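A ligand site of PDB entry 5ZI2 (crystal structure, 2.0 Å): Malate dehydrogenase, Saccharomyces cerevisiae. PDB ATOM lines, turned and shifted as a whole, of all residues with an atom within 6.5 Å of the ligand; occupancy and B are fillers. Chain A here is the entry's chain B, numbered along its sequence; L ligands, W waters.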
ATOM      1  N   LEU A   9       2.168  19.480  20.438  1.00  0.00           N
ATOM      2  CA  LEU A   9       3.615  19.463  20.780  1.00  0.00           C
ATOM      3  C   LEU A   9       3.729  20.020  22.193  1.00  0.00           C
ATOM      4  O   LEU A   9       3.478  21.171  22.442  1.00  0.00           O
ATOM      5  CB  LEU A   9       4.387  20.347  19.765  1.00  0.00           C
ATOM      6  CG  LEU A   9       4.166  20.200  18.277  1.00  0.00           C
ATOM      7  CD1 LEU A   9       5.048  21.123  17.442  1.00  0.00           C
ATOM      8  CD2 LEU A   9       4.406  18.780  17.871  1.00  0.00           C
ATOM      9  N   GLY A  10       4.183  19.171  23.104  1.00  0.00           N
ATOM     10  CA  GLY A  10       4.133  19.389  24.516  1.00  0.00           C
ATOM     11  C   GLY A  10       2.961  18.698  25.160  1.00  0.00           C
ATOM     12  O   GLY A  10       2.445  19.233  26.154  1.00  0.00           O
ATOM     13  N   ALA A  11       2.574  17.507  24.668  1.00  0.00           N
ATOM     14  CA  ALA A  11       1.248  16.895  25.055  1.00  0.00           C
ATOM     15  C   ALA A  11       1.269  16.249  26.442  1.00  0.00           C
ATOM     16  O   ALA A  11       0.216  15.940  26.940  1.00  0.00           O
ATOM     17  CB  ALA A  11       0.795  15.892  24.064  1.00  0.00           C
ATOM     18  N   SER A  12       2.469  16.028  27.034  1.00  0.00           N
ATOM     19  CA  SER A  12       2.579  15.384  28.300  1.00  0.00           C
ATOM     20  C   SER A  12       2.551  16.273  29.475  1.00  0.00           C
ATOM     21  O   SER A  12       2.503  15.791  30.562  1.00  0.00           O
ATOM     22  CB  SER A  12       3.825  14.530  28.320  1.00  0.00           C
ATOM     23  OG  SER A  12       3.770  13.629  27.217  1.00  0.00           O
ATOM     24  N   GLY A  13       2.499  17.580  29.269  1.00  0.00           N
ATOM     25  CA  GLY A  13       2.628  18.510  30.357  1.00  0.00           C
ATOM     26  C   GLY A  13       1.362  18.756  31.104  1.00  0.00           C
ATOM     27  O   GLY A  13       0.284  18.189  30.775  1.00  0.00           O
ATOM     28  N   GLY A  14       1.453  19.653  32.086  1.00  0.00           N
ATOM     29  CA  GLY A  14       0.288  20.028  32.860  1.00  0.00           C
ATOM     30  C   GLY A  14      -0.883  20.550  32.031  1.00  0.00           C
ATOM     31  O   GLY A  14      -2.029  20.185  32.265  1.00  0.00           O
ATOM     32  N   VAL A  15      -0.598  21.394  31.047  1.00  0.00           N
ATOM     33  CA  VAL A  15      -1.646  21.899  30.167  1.00  0.00           C
ATOM     34  C   VAL A  15      -1.878  20.856  29.052  1.00  0.00           C
ATOM     35  O   VAL A  15      -3.006  20.620  28.637  1.00  0.00           O
ATOM     36  CB  VAL A  15      -1.242  23.243  29.507  1.00  0.00           C
ATOM     37  CG1 VAL A  15      -2.270  23.651  28.429  1.00  0.00           C
ATOM     38  CG2 VAL A  15      -1.064  24.389  30.543  1.00  0.00           C
ATOM     39  N   GLY A  16      -0.804  20.323  28.514  1.00  0.00           N
ATOM     40  CA  GLY A  16      -0.909  19.407  27.374  1.00  0.00           C
ATOM     41  C   GLY A  16      -1.771  18.187  27.574  1.00  0.00           C
ATOM     42  O   GLY A  16      -2.460  17.744  26.627  1.00  0.00           O
ATOM     43  N   TYR A  35       2.986  14.588  20.866  1.00  0.00           N
ATOM     44  CA  TYR A  35       4.416  14.554  20.886  1.00  0.00           C
ATOM     45  C   TYR A  35       4.885  15.261  22.098  1.00  0.00           C
ATOM     46  O   TYR A  35       4.270  16.240  22.553  1.00  0.00           O
ATOM     47  CB  TYR A  35       4.948  15.309  19.640  1.00  0.00           C
ATOM     48  CG  TYR A  35       6.390  15.517  19.722  1.00  0.00           C
ATOM     49  CD1 TYR A  35       7.271  14.492  19.312  1.00  0.00           C
ATOM     50  CD2 TYR A  35       6.926  16.703  20.207  1.00  0.00           C
ATOM     51  CE1 TYR A  35       8.636  14.657  19.423  1.00  0.00           C
ATOM     52  CE2 TYR A  35       8.308  16.856  20.339  1.00  0.00           C
ATOM     53  CZ  TYR A  35       9.140  15.818  19.922  1.00  0.00           C
ATOM     54  OH  TYR A  35      10.508  15.997  20.020  1.00  0.00           O
ATOM     55  N   ASP A  36       6.014  14.798  22.617  1.00  0.00           N
ATOM     56  CA  ASP A  36       6.640  15.411  23.769  1.00  0.00           C
ATOM     57  C   ASP A  36       8.031  14.770  23.945  1.00  0.00           C
ATOM     58  O   ASP A  36       8.381  13.722  23.353  1.00  0.00           O
ATOM     59  CB  ASP A  36       5.787  15.212  25.026  1.00  0.00           C
ATOM     60  CG  ASP A  36       6.141  16.184  26.151  1.00  0.00           C
ATOM     61  OD1 ASP A  36       7.331  16.193  26.569  1.00  0.00           O
ATOM     62  OD2 ASP A  36       5.264  16.985  26.613  1.00  0.00           O
ATOM     63  N   ILE A  37       8.878  15.419  24.727  1.00  0.00           N
ATOM     64  CA  ILE A  37      10.207  14.822  24.918  1.00  0.00           C
ATOM     65  C   ILE A  37      10.079  13.590  25.799  1.00  0.00           C
ATOM     66  O   ILE A  37      10.899  12.729  25.698  1.00  0.00           O
ATOM     67  CB  ILE A  37      11.217  15.812  25.495  1.00  0.00           C
ATOM     68  CG1 ILE A  37      10.779  16.297  26.884  1.00  0.00           C
ATOM     69  CG2 ILE A  37      11.459  16.979  24.503  1.00  0.00           C
ATOM     70  CD1 ILE A  37      11.922  17.016  27.561  1.00  0.00           C
ATOM     71  N   ARG A  38       9.024  13.503  26.629  1.00  0.00           N
ATOM     72  CA  ARG A  38       8.730  12.295  27.422  1.00  0.00           C
ATOM     73  C   ARG A  38       7.230  11.909  27.439  1.00  0.00           C
ATOM     74  O   ARG A  38       6.370  12.793  27.416  1.00  0.00           O
ATOM     75  CB  ARG A  38       9.214  12.483  28.855  1.00  0.00           C
ATOM     76  CG  ARG A  38       8.651  13.715  29.584  1.00  0.00           C
ATOM     77  CD  ARG A  38       8.992  13.757  31.104  1.00  0.00           C
ATOM     78  NE  ARG A  38       8.421  12.556  31.732  1.00  0.00           N
ATOM     79  CZ  ARG A  38       7.145  12.401  32.127  1.00  0.00           C
ATOM     80  NH1 ARG A  38       6.790  11.223  32.620  1.00  0.00           N
ATOM     81  NH2 ARG A  38       6.232  13.387  32.026  1.00  0.00           N
ATOM     82  N   ILE A  64       9.281  13.637  15.882  1.00  0.00           N
ATOM     83  CA  ILE A  64       8.506  14.825  15.580  1.00  0.00           C
ATOM     84  C   ILE A  64       8.037  14.908  14.113  1.00  0.00           C
ATOM     85  O   ILE A  64       6.927  15.404  13.835  1.00  0.00           O
ATOM     86  CB  ILE A  64       9.190  16.127  16.047  1.00  0.00           C
ATOM     87  CG1 ILE A  64       8.112  17.205  16.211  1.00  0.00           C
ATOM     88  CG2 ILE A  64      10.294  16.578  15.140  1.00  0.00           C
ATOM     89  CD1 ILE A  64       8.599  18.433  16.880  1.00  0.00           C
ATOM     90  N   PRO A  77       1.465  23.771  23.501  1.00  0.00           N
ATOM     91  CA  PRO A  77       1.479  24.166  24.897  1.00  0.00           C
ATOM     92  C   PRO A  77       2.827  23.772  25.531  1.00  0.00           C
ATOM     93  O   PRO A  77       2.976  23.851  26.763  1.00  0.00           O
ATOM     94  CB  PRO A  77       0.386  23.310  25.495  1.00  0.00           C
ATOM     95  CG  PRO A  77       0.419  22.070  24.711  1.00  0.00           C
ATOM     96  CD  PRO A  77       0.724  22.510  23.310  1.00  0.00           C
ATOM     97  N   ALA A  78       3.809  23.376  24.747  1.00  0.00           N
ATOM     98  CA  ALA A  78       5.107  22.994  25.329  1.00  0.00           C
ATOM     99  C   ALA A  78       5.747  24.153  26.083  1.00  0.00           C
ATOM    100  O   ALA A  78       5.581  25.315  25.722  1.00  0.00           O
ATOM    101  CB  ALA A  78       6.041  22.522  24.245  1.00  0.00           C
ATOM    102  N   GLY A  79       6.537  23.862  27.093  1.00  0.00           N
ATOM    103  CA  GLY A  79       7.142  24.967  27.846  1.00  0.00           C
ATOM    104  C   GLY A  79       7.718  24.464  29.145  1.00  0.00           C
ATOM    105  O   GLY A  79       7.518  23.314  29.454  1.00  0.00           O
ATOM    106  N   VAL A  80       8.478  25.271  29.866  1.00  0.00           N
ATOM    107  CA  VAL A  80       8.919  24.804  31.175  1.00  0.00           C
ATOM    108  C   VAL A  80       8.086  25.493  32.245  1.00  0.00           C
ATOM    109  O   VAL A  80       7.812  26.695  32.124  1.00  0.00           O
ATOM    110  CB  VAL A  80      10.425  24.983  31.476  1.00  0.00           C
ATOM    111  CG1 VAL A  80      11.256  24.402  30.327  1.00  0.00           C
ATOM    112  CG2 VAL A  80      10.765  26.432  31.761  1.00  0.00           C
ATOM    113  N   PRO A  81       7.737  24.746  33.295  1.00  0.00           N
ATOM    114  CA  PRO A  81       6.994  25.271  34.421  1.00  0.00           C
ATOM    115  C   PRO A  81       7.988  25.933  35.446  1.00  0.00           C
ATOM    116  O   PRO A  81       9.143  25.444  35.641  1.00  0.00           O
ATOM    117  CB  PRO A  81       6.390  23.986  35.019  1.00  0.00           C
ATOM    118  CG  PRO A  81       7.531  22.982  34.894  1.00  0.00           C
ATOM    119  CD  PRO A  81       8.309  23.409  33.644  1.00  0.00           C
ATOM    120  N   ASN A  95      11.654  28.829  27.266  1.00  0.00           N
ATOM    121  CA  ASN A  95      10.427  28.693  26.501  1.00  0.00           C
ATOM    122  C   ASN A  95      10.591  29.230  25.070  1.00  0.00           C
ATOM    123  O   ASN A  95      10.002  28.698  24.111  1.00  0.00           O
ATOM    124  CB  ASN A  95       9.266  29.393  27.221  1.00  0.00           C
ATOM    125  CG  ASN A  95       8.615  28.517  28.250  1.00  0.00           C
ATOM    126  OD1 ASN A  95       9.058  27.412  28.464  1.00  0.00           O
ATOM    127  ND2 ASN A  95       7.539  28.990  28.855  1.00  0.00           N
ATOM    128  N   GLY A  97      13.529  29.191  23.490  1.00  0.00           N
ATOM    129  CA  GLY A  97      14.246  28.073  22.827  1.00  0.00           C
ATOM    130  C   GLY A  97      13.370  26.896  22.416  1.00  0.00           C
ATOM    131  O   GLY A  97      13.517  26.361  21.317  1.00  0.00           O
ATOM    132  N   ILE A  98      12.452  26.484  23.282  1.00  0.00           N
ATOM    133  CA  ILE A  98      11.480  25.396  22.979  1.00  0.00           C
ATOM    134  C   ILE A  98      10.597  25.803  21.731  1.00  0.00           C
ATOM    135  O   ILE A  98      10.474  25.031  20.765  1.00  0.00           O
ATOM    136  CB  ILE A  98      10.583  25.119  24.210  1.00  0.00           C
ATOM    137  CG1 ILE A  98      11.386  24.363  25.283  1.00  0.00           C
ATOM    138  CG2 ILE A  98       9.316  24.355  23.830  1.00  0.00           C
ATOM    139  CD1 ILE A  98      10.852  24.545  26.675  1.00  0.00           C
ATOM    140  N   VAL A  99       9.962  26.976  21.812  1.00  0.00           N
ATOM    141  CA  VAL A  99       9.122  27.519  20.712  1.00  0.00           C
ATOM    142  C   VAL A  99       9.863  27.651  19.402  1.00  0.00           C
ATOM    143  O   VAL A  99       9.332  27.261  18.323  1.00  0.00           O
ATOM    144  CB  VAL A  99       8.445  28.838  21.115  1.00  0.00           C
ATOM    145  CG1 VAL A  99       7.772  29.551  19.943  1.00  0.00           C
ATOM    146  CG2 VAL A  99       7.396  28.533  22.197  1.00  0.00           C
ATOM    147  N   SER A 101      12.444  25.943  18.434  1.00  0.00           N
ATOM    148  CA  SER A 101      12.739  24.620  17.975  1.00  0.00           C
ATOM    149  C   SER A 101      11.498  23.913  17.446  1.00  0.00           C
ATOM    150  O   SER A 101      11.571  23.234  16.448  1.00  0.00           O
ATOM    151  CB  SER A 101      13.297  23.858  19.166  1.00  0.00           C
ATOM    152  OG  SER A 101      13.573  22.596  18.707  1.00  0.00           O
ATOM    153  N   LEU A 102      10.366  24.044  18.149  1.00  0.00           N
ATOM    154  CA  LEU A 102       9.141  23.380  17.689  1.00  0.00           C
ATOM    155  C   LEU A 102       8.602  23.971  16.369  1.00  0.00           C
ATOM    156  O   LEU A 102       8.144  23.247  15.515  1.00  0.00           O
ATOM    157  CB  LEU A 102       8.074  23.337  18.780  1.00  0.00           C
ATOM    158  CG  LEU A 102       8.514  22.432  19.940  1.00  0.00           C
ATOM    159  CD1 LEU A 102       7.604  22.705  21.105  1.00  0.00           C
ATOM    160  CD2 LEU A 102       8.616  20.937  19.605  1.00  0.00           C
ATOM    161  N   SER A 234       0.336  27.173  38.037  1.00  0.00           N
ATOM    162  CA  SER A 234      -0.526  28.205  37.462  1.00  0.00           C
ATOM    163  C   SER A 234      -1.732  27.508  36.810  1.00  0.00           C
ATOM    164  O   SER A 234      -1.937  26.361  37.066  1.00  0.00           O
ATOM    165  CB  SER A 234       0.261  29.071  36.475  1.00  0.00           C
ATOM    166  OG  SER A 234       1.141  28.259  35.725  1.00  0.00           O
ATOM    167  N   ALA A 235      -2.569  28.233  36.075  1.00  0.00           N
ATOM    168  CA  ALA A 235      -3.761  27.651  35.505  1.00  0.00           C
ATOM    169  C   ALA A 235      -3.308  26.607  34.493  1.00  0.00           C
ATOM    170  O   ALA A 235      -2.501  26.890  33.597  1.00  0.00           O
ATOM    171  CB  ALA A 235      -4.587  28.738  34.850  1.00  0.00           C
ATOM    172  N   THR A 236      -3.693  25.373  34.720  1.00  0.00           N
ATOM    173  CA  THR A 236      -3.473  24.279  33.772  1.00  0.00           C
ATOM    174  C   THR A 236      -4.786  23.875  33.100  1.00  0.00           C
ATOM    175  O   THR A 236      -4.862  23.851  31.918  1.00  0.00           O
ATOM    176  CB  THR A 236      -2.896  23.072  34.466  1.00  0.00           C
ATOM    177  OG1 THR A 236      -3.763  22.701  35.532  1.00  0.00           O
ATOM    178  CG2 THR A 236      -1.517  23.429  35.079  1.00  0.00           C
HETATM  179  P1  LIG L   1       2.678  23.490  31.777  1.00  0.00           P
HETATM  180  O1  LIG L   1       3.511  24.628  31.149  1.00  0.00           O
HETATM  181  O2  LIG L   1       1.803  24.000  32.893  1.00  0.00           O
HETATM  182  O3  LIG L   1       1.881  22.628  30.818  1.00  0.00           O
HETATM  183  P2  LIG L   1       4.681  21.353  32.311  1.00  0.00           P
HETATM  184  O4  LIG L   1       6.180  21.469  32.524  1.00  0.00           O
HETATM  185  O5  LIG L   1       3.882  20.444  33.215  1.00  0.00           O
HETATM  186  O6  LIG L   1       3.958  22.776  32.431  1.00  0.00           O
HETATM  187  O7  LIG L   1       4.454  20.909  30.764  1.00  0.00           O
HETATM  188  C1  LIG L   1       5.249  21.294  29.617  1.00  0.00           C
HETATM  189  C2  LIG L   1       5.515  20.119  28.657  1.00  0.00           C
HETATM  190  O8  LIG L   1       6.326  20.553  27.573  1.00  0.00           O
HETATM  191  C3  LIG L   1       6.268  18.983  29.365  1.00  0.00           C
HETATM  192  O9  LIG L   1       5.543  17.753  29.178  1.00  0.00           O
HETATM  193  C4  LIG L   1       7.651  18.945  28.764  1.00  0.00           C
HETATM  194  O10 LIG L   1       8.260  17.632  28.658  1.00  0.00           O
HETATM  195  C5  LIG L   1       7.291  19.524  27.380  1.00  0.00           C
HETATM  196  N1  LIG L   1       8.457  20.013  26.601  1.00  0.00           N
HETATM  197  C6  LIG L   1       9.516  20.720  27.031  1.00  0.00           C
HETATM  198  N2  LIG L   1      10.329  20.942  25.969  1.00  0.00           N
HETATM  199  C7  LIG L   1       9.815  20.395  24.870  1.00  0.00           C
HETATM  200  C8  LIG L   1      10.184  20.263  23.442  1.00  0.00           C
HETATM  201  N3  LIG L   1      11.299  20.799  22.919  1.00  0.00           N
HETATM  202  N4  LIG L   1       9.341  19.613  22.646  1.00  0.00           N
HETATM  203  C9  LIG L   1       8.185  19.061  23.105  1.00  0.00           C
HETATM  204  N5  LIG L   1       7.823  19.121  24.398  1.00  0.00           N
HETATM  205  C10 LIG L   1       8.571  19.781  25.298  1.00  0.00           C
HETATM  206  O   HOH W   1       6.209  16.239  31.092  1.00  0.00           O
HETATM  207  O   HOH W   2      12.141  20.514  19.797  1.00  0.00           O
HETATM  208  O   HOH W   3       1.969  21.102  28.352  1.00  0.00           O
HETATM  209  O   HOH W   4      12.752  21.397  26.989  1.00  0.00           O
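The side-chain carboxylate (OD2) of Asp 36 lies within hydrogen-bond range of an oxygen (O9) of the ligand (2.7 Å). An oxygen (O3) of the ligand sits at hydrogen-bond distance from the backbone NH (N) of Val 15 (2.8 Å). N of Gly 14 lies within hydrogen-bond range of O5 of the ligand. An oxygen (O8) of the ligand lies within hydrogen-bond range of the backbone NH (N) of Gly 79 (3.4 Å). O9 of the ligand is in hydrogen-bond range of N of Gly 13 (3.1 Å).
Water W1 bridges O9 of the ligand (2.5 Å) and NH2 of Arg 38 (3.0 Å). Water W3 lies within hydrogen-bond range of the backbone NH of Gly 16 (2.9 Å), an oxygen (O3) of the ligand (2.9 Å), the backbone carbonyl oxygen of Gly 10 (2.9 Å) and the backbone carbonyl oxygen of Pro 77 (3.3 Å). Water W2 lies within hydrogen-bond range of the side-chain hydroxyl of Ser 101 and a nitrogen (N3) of the ligand.
The side-chain carboxylate (OD2) of Asp 36 is in hydrogen-bond range of the backbone NH (N) of Ser 12 (3.0 Å). The backbone NH (N) of Arg 38 sits close to the side-chain carboxylate (OD1) of Asp 36 (3.2 Å). OD2 of Asp 36 lies within hydrogen-bond range of N of Ala 11 (3.4 Å). O of Arg 38 lies within hydrogen-bond range of OG of Ser 12, at 2.7 Å. The backbone carbonyl oxygen of Leu 9 is in hydrogen-bond range of the backbone NH of Ala 78 (3.2 Å). The backbone carbonyl oxygen of Tyr 35 lies within hydrogen-bond range of the backbone NH of Gly 10. O of Tyr 35 is in hydrogen-bond range of N of Ala 11.
Merely in contact with the ligand: Gly 10, Ser 12, Tyr 35, Ile 37, Ala 78, Pro 81, Ile 98 and Leu 102. Hydrophobic or aromatic side chains within 4 Å of the ligand: Val 15, Tyr 35, Ile 37, Ala 78, Pro 81, Ile 98 and Leu 102. Within 4 Å of the ligand: Gly 10, Ser 12, Gly 13, Gly 14, Val 15, Tyr 35, Asp 36, Ile 37, Ala 78, Gly 79, Pro 81, Ile 98 and Leu 102.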
